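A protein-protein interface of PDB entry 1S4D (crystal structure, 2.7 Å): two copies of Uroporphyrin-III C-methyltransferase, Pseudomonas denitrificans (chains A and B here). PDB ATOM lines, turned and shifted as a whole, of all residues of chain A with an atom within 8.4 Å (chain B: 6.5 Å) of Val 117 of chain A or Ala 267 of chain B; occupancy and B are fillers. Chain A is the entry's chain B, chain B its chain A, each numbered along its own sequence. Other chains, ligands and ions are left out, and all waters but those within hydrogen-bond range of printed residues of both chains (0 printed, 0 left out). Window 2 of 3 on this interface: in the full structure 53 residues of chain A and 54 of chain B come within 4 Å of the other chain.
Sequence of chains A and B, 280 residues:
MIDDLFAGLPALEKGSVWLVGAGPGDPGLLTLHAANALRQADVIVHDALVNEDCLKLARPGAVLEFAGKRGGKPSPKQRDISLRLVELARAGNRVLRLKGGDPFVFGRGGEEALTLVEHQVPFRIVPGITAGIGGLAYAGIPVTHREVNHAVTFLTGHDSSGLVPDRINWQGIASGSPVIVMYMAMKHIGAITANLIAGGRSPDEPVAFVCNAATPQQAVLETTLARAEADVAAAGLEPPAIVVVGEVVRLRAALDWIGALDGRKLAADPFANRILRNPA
N of Ala 267 of chain B is in hydrogen-bond range of O of Ala 253 of chain B.
CD2 of Leu 255 of chain B touches CB of Ala 113 of chain A, at 3.6 Å. Leu 114 of chain A touches Ala 254 of chain B (CD1 to CB, 3.9 Å). Leu 255 of chain B touches Leu 114 of chain A (CD2 to CD1, 3.6 Å). CD2 of Leu 114 of chain A touches CG of Asp 269 of chain B (3.6 Å). Val 117 of chain A touches Ala 254 of chain B (CG2 to O, 3.5 Å). CG1 of Val 117 of chain A touches CB of Leu 266 of chain B (3.8 Å). CG1 of Val 117 of chain A touches O of Ala 267 of chain B (3.7 Å). O of Leu 255 of chain B touches CZ of Phe 123 of chain A, at 3.95 Å.
Val 86 of chain A touches none of the printed residues of chain B. Of the printed residues of chain B, Leu 114 of chain A touches Ala 254 (3.9 Å), Leu 255 (3.6 Å) and Asp 269 (3.6 Å). Val 117 of chain A touches just these residues of chain B: Ala 254, Leu 266 and Ala 267. His 119 of chain A touches none of the printed residues of chain B. Of the printed residues of chain A, Leu 266 of chain B touches Val 117 (3.8 Å). Ala 268 of chain B touches none of the printed residues of chain A. The nearest residue of chain B that does not touch Val 117 of chain A is Leu 255 of chain B (4.6 Å).
Of the 16 printed residues of chain A, 4 touch a printed residue of chain B. Of the 8 printed residues of chain B, 5 touch a printed residue of chain A. Hydrophobic or aromatic side chains of chain B within 4 Å of the printed part of chain A: Ala 254, Leu 255 and Leu 266.
No position is printed for both chains. Of the 8 pairs that touch across the chains among the printed residues, none has its exchanged pair printed and touching as well.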
ATOM      1  N   VAL A  86      -2.912  -8.529 -18.123  1.00  0.00           N
ATOM      2  CA  VAL A  86      -3.721  -8.388 -19.311  1.00  0.00           C
ATOM      3  C   VAL A  86      -2.950  -7.610 -20.389  1.00  0.00           C
ATOM      4  O   VAL A  86      -3.017  -7.953 -21.566  1.00  0.00           O
ATOM      5  CB  VAL A  86      -5.095  -7.736 -18.976  1.00  0.00           C
ATOM      6  CG1 VAL A  86      -5.866  -7.317 -20.251  1.00  0.00           C
ATOM      7  CG2 VAL A  86      -5.932  -8.686 -18.124  1.00  0.00           C
ATOM      8  N   ARG A  90      -2.186  -9.295 -24.007  1.00  0.00           N
ATOM      9  CA  ARG A  90      -2.697  -8.656 -25.214  1.00  0.00           C
ATOM     10  C   ARG A  90      -1.584  -8.273 -26.214  1.00  0.00           C
ATOM     11  O   ARG A  90      -1.812  -8.215 -27.411  1.00  0.00           O
ATOM     12  CB  ARG A  90      -3.549  -7.430 -24.858  1.00  0.00           C
ATOM     13  CG  ARG A  90      -4.912  -7.777 -24.303  1.00  0.00           C
ATOM     14  CD  ARG A  90      -5.903  -6.619 -24.305  1.00  0.00           C
ATOM     15  NE  ARG A  90      -7.265  -7.097 -24.066  1.00  0.00           N
ATOM     16  CZ  ARG A  90      -8.209  -6.400 -23.449  1.00  0.00           C
ATOM     17  NH1 ARG A  90      -7.965  -5.175 -23.001  1.00  0.00           N
ATOM     18  NH2 ARG A  90      -9.405  -6.935 -23.271  1.00  0.00           N
ATOM     19  N   GLY A 110      -7.601 -16.245  -7.577  1.00  0.00           N
ATOM     20  CA  GLY A 110      -8.964 -16.103  -8.064  1.00  0.00           C
ATOM     21  C   GLY A 110      -9.256 -14.736  -8.658  1.00  0.00           C
ATOM     22  O   GLY A 110      -9.760 -14.658  -9.780  1.00  0.00           O
ATOM     23  N   GLU A 111      -8.925 -13.667  -7.932  1.00  0.00           N
ATOM     24  CA  GLU A 111      -9.115 -12.305  -8.433  1.00  0.00           C
ATOM     25  C   GLU A 111      -8.392 -12.116  -9.759  1.00  0.00           C
ATOM     26  O   GLU A 111      -8.986 -11.621 -10.728  1.00  0.00           O
ATOM     27  CB  GLU A 111      -8.617 -11.258  -7.440  1.00  0.00           C
ATOM     28  CG  GLU A 111      -9.484 -11.154  -6.211  1.00  0.00           C
ATOM     29  CD  GLU A 111      -8.939 -10.184  -5.178  1.00  0.00           C
ATOM     30  OE1 GLU A 111      -8.388 -10.651  -4.147  1.00  0.00           O
ATOM     31  OE2 GLU A 111      -9.075  -8.949  -5.405  1.00  0.00           O
ATOM     32  N   GLU A 112      -7.113 -12.509  -9.798  1.00  0.00           N
ATOM     33  CA  GLU A 112      -6.325 -12.350 -11.014  1.00  0.00           C
ATOM     34  C   GLU A 112      -7.006 -13.063 -12.185  1.00  0.00           C
ATOM     35  O   GLU A 112      -7.290 -12.417 -13.202  1.00  0.00           O
ATOM     36  CB  GLU A 112      -4.897 -12.825 -10.814  1.00  0.00           C
ATOM     37  CG  GLU A 112      -4.158 -11.946  -9.833  1.00  0.00           C
ATOM     38  CD  GLU A 112      -2.709 -12.317  -9.610  1.00  0.00           C
ATOM     39  OE1 GLU A 112      -2.377 -13.521  -9.441  1.00  0.00           O
ATOM     40  OE2 GLU A 112      -1.916 -11.367  -9.565  1.00  0.00           O
ATOM     41  N   ALA A 113      -7.305 -14.359 -12.025  1.00  0.00           N
ATOM     42  CA  ALA A 113      -7.944 -15.141 -13.069  1.00  0.00           C
ATOM     43  C   ALA A 113      -9.244 -14.473 -13.504  1.00  0.00           C
ATOM     44  O   ALA A 113      -9.539 -14.380 -14.693  1.00  0.00           O
ATOM     45  CB  ALA A 113      -8.204 -16.580 -12.584  1.00  0.00           C
ATOM     46  N   LEU A 114     -10.002 -13.981 -12.528  1.00  0.00           N
ATOM     47  CA  LEU A 114     -11.276 -13.324 -12.809  1.00  0.00           C
ATOM     48  C   LEU A 114     -11.059 -12.111 -13.697  1.00  0.00           C
ATOM     49  O   LEU A 114     -11.802 -11.893 -14.656  1.00  0.00           O
ATOM     50  CB  LEU A 114     -11.945 -12.912 -11.512  1.00  0.00           C
ATOM     51  CG  LEU A 114     -13.348 -13.380 -11.128  1.00  0.00           C
ATOM     52  CD1 LEU A 114     -13.733 -14.773 -11.642  1.00  0.00           C
ATOM     53  CD2 LEU A 114     -13.495 -13.276  -9.591  1.00  0.00           C
ATOM     54  N   THR A 115     -10.021 -11.339 -13.399  1.00  0.00           N
ATOM     55  CA  THR A 115      -9.651 -10.215 -14.236  1.00  0.00           C
ATOM     56  C   THR A 115      -9.246 -10.701 -15.624  1.00  0.00           C
ATOM     57  O   THR A 115      -9.693 -10.142 -16.632  1.00  0.00           O
ATOM     58  CB  THR A 115      -8.525  -9.399 -13.579  1.00  0.00           C
ATOM     59  OG1 THR A 115      -8.973  -8.919 -12.305  1.00  0.00           O
ATOM     60  CG2 THR A 115      -8.260  -8.123 -14.355  1.00  0.00           C
ATOM     61  N   LEU A 116      -8.421 -11.749 -15.679  1.00  0.00           N
ATOM     62  CA  LEU A 116      -8.060 -12.358 -16.964  1.00  0.00           C
ATOM     63  C   LEU A 116      -9.322 -12.703 -17.814  1.00  0.00           C
ATOM     64  O   LEU A 116      -9.432 -12.291 -18.971  1.00  0.00           O
ATOM     65  CB  LEU A 116      -7.141 -13.564 -16.755  1.00  0.00           C
ATOM     66  CG  LEU A 116      -5.599 -13.412 -16.729  1.00  0.00           C
ATOM     67  CD1 LEU A 116      -5.062 -11.990 -16.888  1.00  0.00           C
ATOM     68  CD2 LEU A 116      -4.970 -14.058 -15.508  1.00  0.00           C
ATOM     69  N   VAL A 117     -10.287 -13.404 -17.222  1.00  0.00           N
ATOM     70  CA  VAL A 117     -11.503 -13.770 -17.930  1.00  0.00           C
ATOM     71  C   VAL A 117     -12.276 -12.547 -18.476  1.00  0.00           C
ATOM     72  O   VAL A 117     -12.615 -12.498 -19.662  1.00  0.00           O
ATOM     73  CB  VAL A 117     -12.407 -14.661 -17.065  1.00  0.00           C
ATOM     74  CG1 VAL A 117     -13.758 -14.832 -17.724  1.00  0.00           C
ATOM     75  CG2 VAL A 117     -11.745 -16.007 -16.848  1.00  0.00           C
ATOM     76  N   GLU A 118     -12.522 -11.569 -17.604  1.00  0.00           N
ATOM     77  CA  GLU A 118     -13.172 -10.309 -17.947  1.00  0.00           C
ATOM     78  C   GLU A 118     -12.600  -9.670 -19.223  1.00  0.00           C
ATOM     79  O   GLU A 118     -13.340  -9.096 -20.023  1.00  0.00           O
ATOM     80  CB  GLU A 118     -13.038  -9.364 -16.738  1.00  0.00           C
ATOM     81  CG  GLU A 118     -13.461  -7.902 -16.890  1.00  0.00           C
ATOM     82  CD  GLU A 118     -12.951  -7.058 -15.722  1.00  0.00           C
ATOM     83  OE1 GLU A 118     -12.648  -7.634 -14.644  1.00  0.00           O
ATOM     84  OE2 GLU A 118     -12.824  -5.821 -15.864  1.00  0.00           O
ATOM     85  N   HIS A 119     -11.290  -9.783 -19.417  1.00  0.00           N
ATOM     86  CA  HIS A 119     -10.622  -9.140 -20.547  1.00  0.00           C
ATOM     87  C   HIS A 119     -10.251 -10.132 -21.640  1.00  0.00           C
ATOM     88  O   HIS A 119      -9.409  -9.827 -22.495  1.00  0.00           O
ATOM     89  CB  HIS A 119      -9.376  -8.384 -20.090  1.00  0.00           C
ATOM     90  CG  HIS A 119      -9.639  -7.359 -19.032  1.00  0.00           C
ATOM     91  ND1 HIS A 119      -9.776  -6.015 -19.316  1.00  0.00           N
ATOM     92  CD2 HIS A 119      -9.777  -7.478 -17.691  1.00  0.00           C
ATOM     93  CE1 HIS A 119      -9.997  -5.351 -18.196  1.00  0.00           C
ATOM     94  NE2 HIS A 119      -9.999  -6.215 -17.194  1.00  0.00           N
ATOM     95  N   GLN A 120     -10.879 -11.315 -21.601  1.00  0.00           N
ATOM     96  CA  GLN A 120     -10.778 -12.315 -22.686  1.00  0.00           C
ATOM     97  C   GLN A 120      -9.363 -12.916 -22.835  1.00  0.00           C
ATOM     98  O   GLN A 120      -8.934 -13.262 -23.939  1.00  0.00           O
ATOM     99  CB  GLN A 120     -11.261 -11.738 -24.027  1.00  0.00           C
ATOM    100  CG  GLN A 120     -12.646 -11.136 -24.006  1.00  0.00           C
ATOM    101  CD  GLN A 120     -13.703 -12.186 -24.125  1.00  0.00           C
ATOM    102  OE1 GLN A 120     -14.145 -12.731 -23.118  1.00  0.00           O
ATOM    103  NE2 GLN A 120     -14.107 -12.494 -25.356  1.00  0.00           N
ATOM    104  N   VAL A 121      -8.636 -13.050 -21.731  1.00  0.00           N
ATOM    105  CA  VAL A 121      -7.292 -13.619 -21.801  1.00  0.00           C
ATOM    106  C   VAL A 121      -7.320 -15.056 -21.272  1.00  0.00           C
ATOM    107  O   VAL A 121      -7.741 -15.277 -20.141  1.00  0.00           O
ATOM    108  CB  VAL A 121      -6.292 -12.748 -21.011  1.00  0.00           C
ATOM    109  CG1 VAL A 121      -4.927 -13.393 -20.944  1.00  0.00           C
ATOM    110  CG2 VAL A 121      -6.191 -11.372 -21.627  1.00  0.00           C
ATOM    111  N   PRO A 122      -6.895 -16.046 -22.061  1.00  0.00           N
ATOM    112  CA  PRO A 122      -6.872 -17.432 -21.559  1.00  0.00           C
ATOM    113  C   PRO A 122      -5.792 -17.596 -20.506  1.00  0.00           C
ATOM    114  O   PRO A 122      -4.794 -16.852 -20.519  1.00  0.00           O
ATOM    115  CB  PRO A 122      -6.553 -18.271 -22.800  1.00  0.00           C
ATOM    116  CG  PRO A 122      -5.871 -17.343 -23.737  1.00  0.00           C
ATOM    117  CD  PRO A 122      -6.385 -15.945 -23.441  1.00  0.00           C
ATOM    118  N   PHE A 123      -5.999 -18.548 -19.594  1.00  0.00           N
ATOM    119  CA  PHE A 123      -5.060 -18.795 -18.503  1.00  0.00           C
ATOM    120  C   PHE A 123      -5.093 -20.243 -18.122  1.00  0.00           C
ATOM    121  O   PHE A 123      -6.053 -20.950 -18.418  1.00  0.00           O
ATOM    122  CB  PHE A 123      -5.402 -17.953 -17.269  1.00  0.00           C
ATOM    123  CG  PHE A 123      -6.711 -18.312 -16.646  1.00  0.00           C
ATOM    124  CD1 PHE A 123      -6.767 -19.146 -15.554  1.00  0.00           C
ATOM    125  CD2 PHE A 123      -7.896 -17.806 -17.164  1.00  0.00           C
ATOM    126  CE1 PHE A 123      -7.980 -19.489 -14.989  1.00  0.00           C
ATOM    127  CE2 PHE A 123      -9.121 -18.142 -16.607  1.00  0.00           C
ATOM    128  CZ  PHE A 123      -9.166 -18.993 -15.522  1.00  0.00           C
ATOM    129  N   ALA B 253     -18.028 -21.822 -12.747  1.00  0.00           N
ATOM    130  CA  ALA B 253     -18.559 -21.289 -14.008  1.00  0.00           C
ATOM    131  C   ALA B 253     -17.646 -20.213 -14.620  1.00  0.00           C
ATOM    132  O   ALA B 253     -17.696 -19.955 -15.840  1.00  0.00           O
ATOM    133  CB  ALA B 253     -19.947 -20.750 -13.818  1.00  0.00           C
ATOM    134  N   ALA B 254     -16.803 -19.606 -13.777  1.00  0.00           N
ATOM    135  CA  ALA B 254     -15.940 -18.502 -14.191  1.00  0.00           C
ATOM    136  C   ALA B 254     -14.461 -18.863 -14.280  1.00  0.00           C
ATOM    137  O   ALA B 254     -13.707 -18.182 -14.971  1.00  0.00           O
ATOM    138  CB  ALA B 254     -16.119 -17.321 -13.276  1.00  0.00           C
ATOM    139  N   LEU B 255     -14.025 -19.914 -13.595  1.00  0.00           N
ATOM    140  CA  LEU B 255     -12.592 -20.194 -13.556  1.00  0.00           C
ATOM    141  C   LEU B 255     -12.204 -21.554 -14.094  1.00  0.00           C
ATOM    142  O   LEU B 255     -11.090 -22.021 -13.863  1.00  0.00           O
ATOM    143  CB  LEU B 255     -12.064 -20.032 -12.132  1.00  0.00           C
ATOM    144  CG  LEU B 255     -12.152 -18.628 -11.556  1.00  0.00           C
ATOM    145  CD1 LEU B 255     -11.367 -18.601 -10.264  1.00  0.00           C
ATOM    146  CD2 LEU B 255     -11.648 -17.546 -12.528  1.00  0.00           C
ATOM    147  N   LYS B 265     -17.396 -21.096 -22.427  1.00  0.00           N
ATOM    148  CA  LYS B 265     -17.562 -19.651 -22.286  1.00  0.00           C
ATOM    149  C   LYS B 265     -17.570 -19.303 -20.799  1.00  0.00           C
ATOM    150  O   LYS B 265     -18.558 -19.530 -20.100  1.00  0.00           O
ATOM    151  CB  LYS B 265     -18.878 -19.209 -22.947  1.00  0.00           C
ATOM    152  CG  LYS B 265     -18.751 -18.306 -24.155  1.00  0.00           C
ATOM    153  CD  LYS B 265     -20.136 -18.078 -24.763  1.00  0.00           C
ATOM    154  CE  LYS B 265     -20.095 -17.835 -26.279  1.00  0.00           C
ATOM    155  NZ  LYS B 265     -20.626 -16.478 -26.633  1.00  0.00           N
ATOM    156  N   LEU B 266     -16.454 -18.782 -20.309  1.00  0.00           N
ATOM    157  CA  LEU B 266     -16.316 -18.469 -18.883  1.00  0.00           C
ATOM    158  C   LEU B 266     -17.070 -17.179 -18.517  1.00  0.00           C
ATOM    159  O   LEU B 266     -16.997 -16.191 -19.251  1.00  0.00           O
ATOM    160  CB  LEU B 266     -14.834 -18.386 -18.495  1.00  0.00           C
ATOM    161  CG  LEU B 266     -14.086 -19.546 -17.814  1.00  0.00           C
ATOM    162  CD1 LEU B 266     -14.713 -20.904 -18.038  1.00  0.00           C
ATOM    163  CD2 LEU B 266     -12.619 -19.579 -18.226  1.00  0.00           C
ATOM    164  N   ALA B 267     -17.781 -17.206 -17.385  1.00  0.00           N
ATOM    165  CA  ALA B 267     -18.669 -16.120 -16.951  1.00  0.00           C
ATOM    166  C   ALA B 267     -18.003 -15.147 -15.963  1.00  0.00           C
ATOM    167  O   ALA B 267     -16.801 -15.243 -15.719  1.00  0.00           O
ATOM    168  CB  ALA B 267     -19.936 -16.717 -16.344  1.00  0.00           C
ATOM    169  N   ALA B 268     -18.785 -14.212 -15.407  1.00  0.00           N
ATOM    170  CA  ALA B 268     -18.328 -13.305 -14.333  1.00  0.00           C
ATOM    171  C   ALA B 268     -18.972 -13.669 -12.987  1.00  0.00           C
ATOM    172  O   ALA B 268     -20.106 -14.162 -12.956  1.00  0.00           O
ATOM    173  CB  ALA B 268     -18.619 -11.857 -14.695  1.00  0.00           C
ATOM    174  N   ASP B 269     -18.273 -13.364 -11.887  1.00  0.00           N
ATOM    175  CA  ASP B 269     -18.442 -14.069 -10.586  1.00  0.00           C
ATOM    176  C   ASP B 269     -19.849 -14.323  -9.984  1.00  0.00           C
ATOM    177  O   ASP B 269     -20.345 -15.442 -10.123  1.00  0.00           O
ATOM    178  CB  ASP B 269     -17.419 -13.610  -9.510  1.00  0.00           C
ATOM    179  CG  ASP B 269     -16.931 -12.160  -9.689  1.00  0.00           C
ATOM    180  OD1 ASP B 269     -16.844 -11.648 -10.831  1.00  0.00           O
ATOM    181  OD2 ASP B 269     -16.586 -11.466  -8.710  1.00  0.00           O
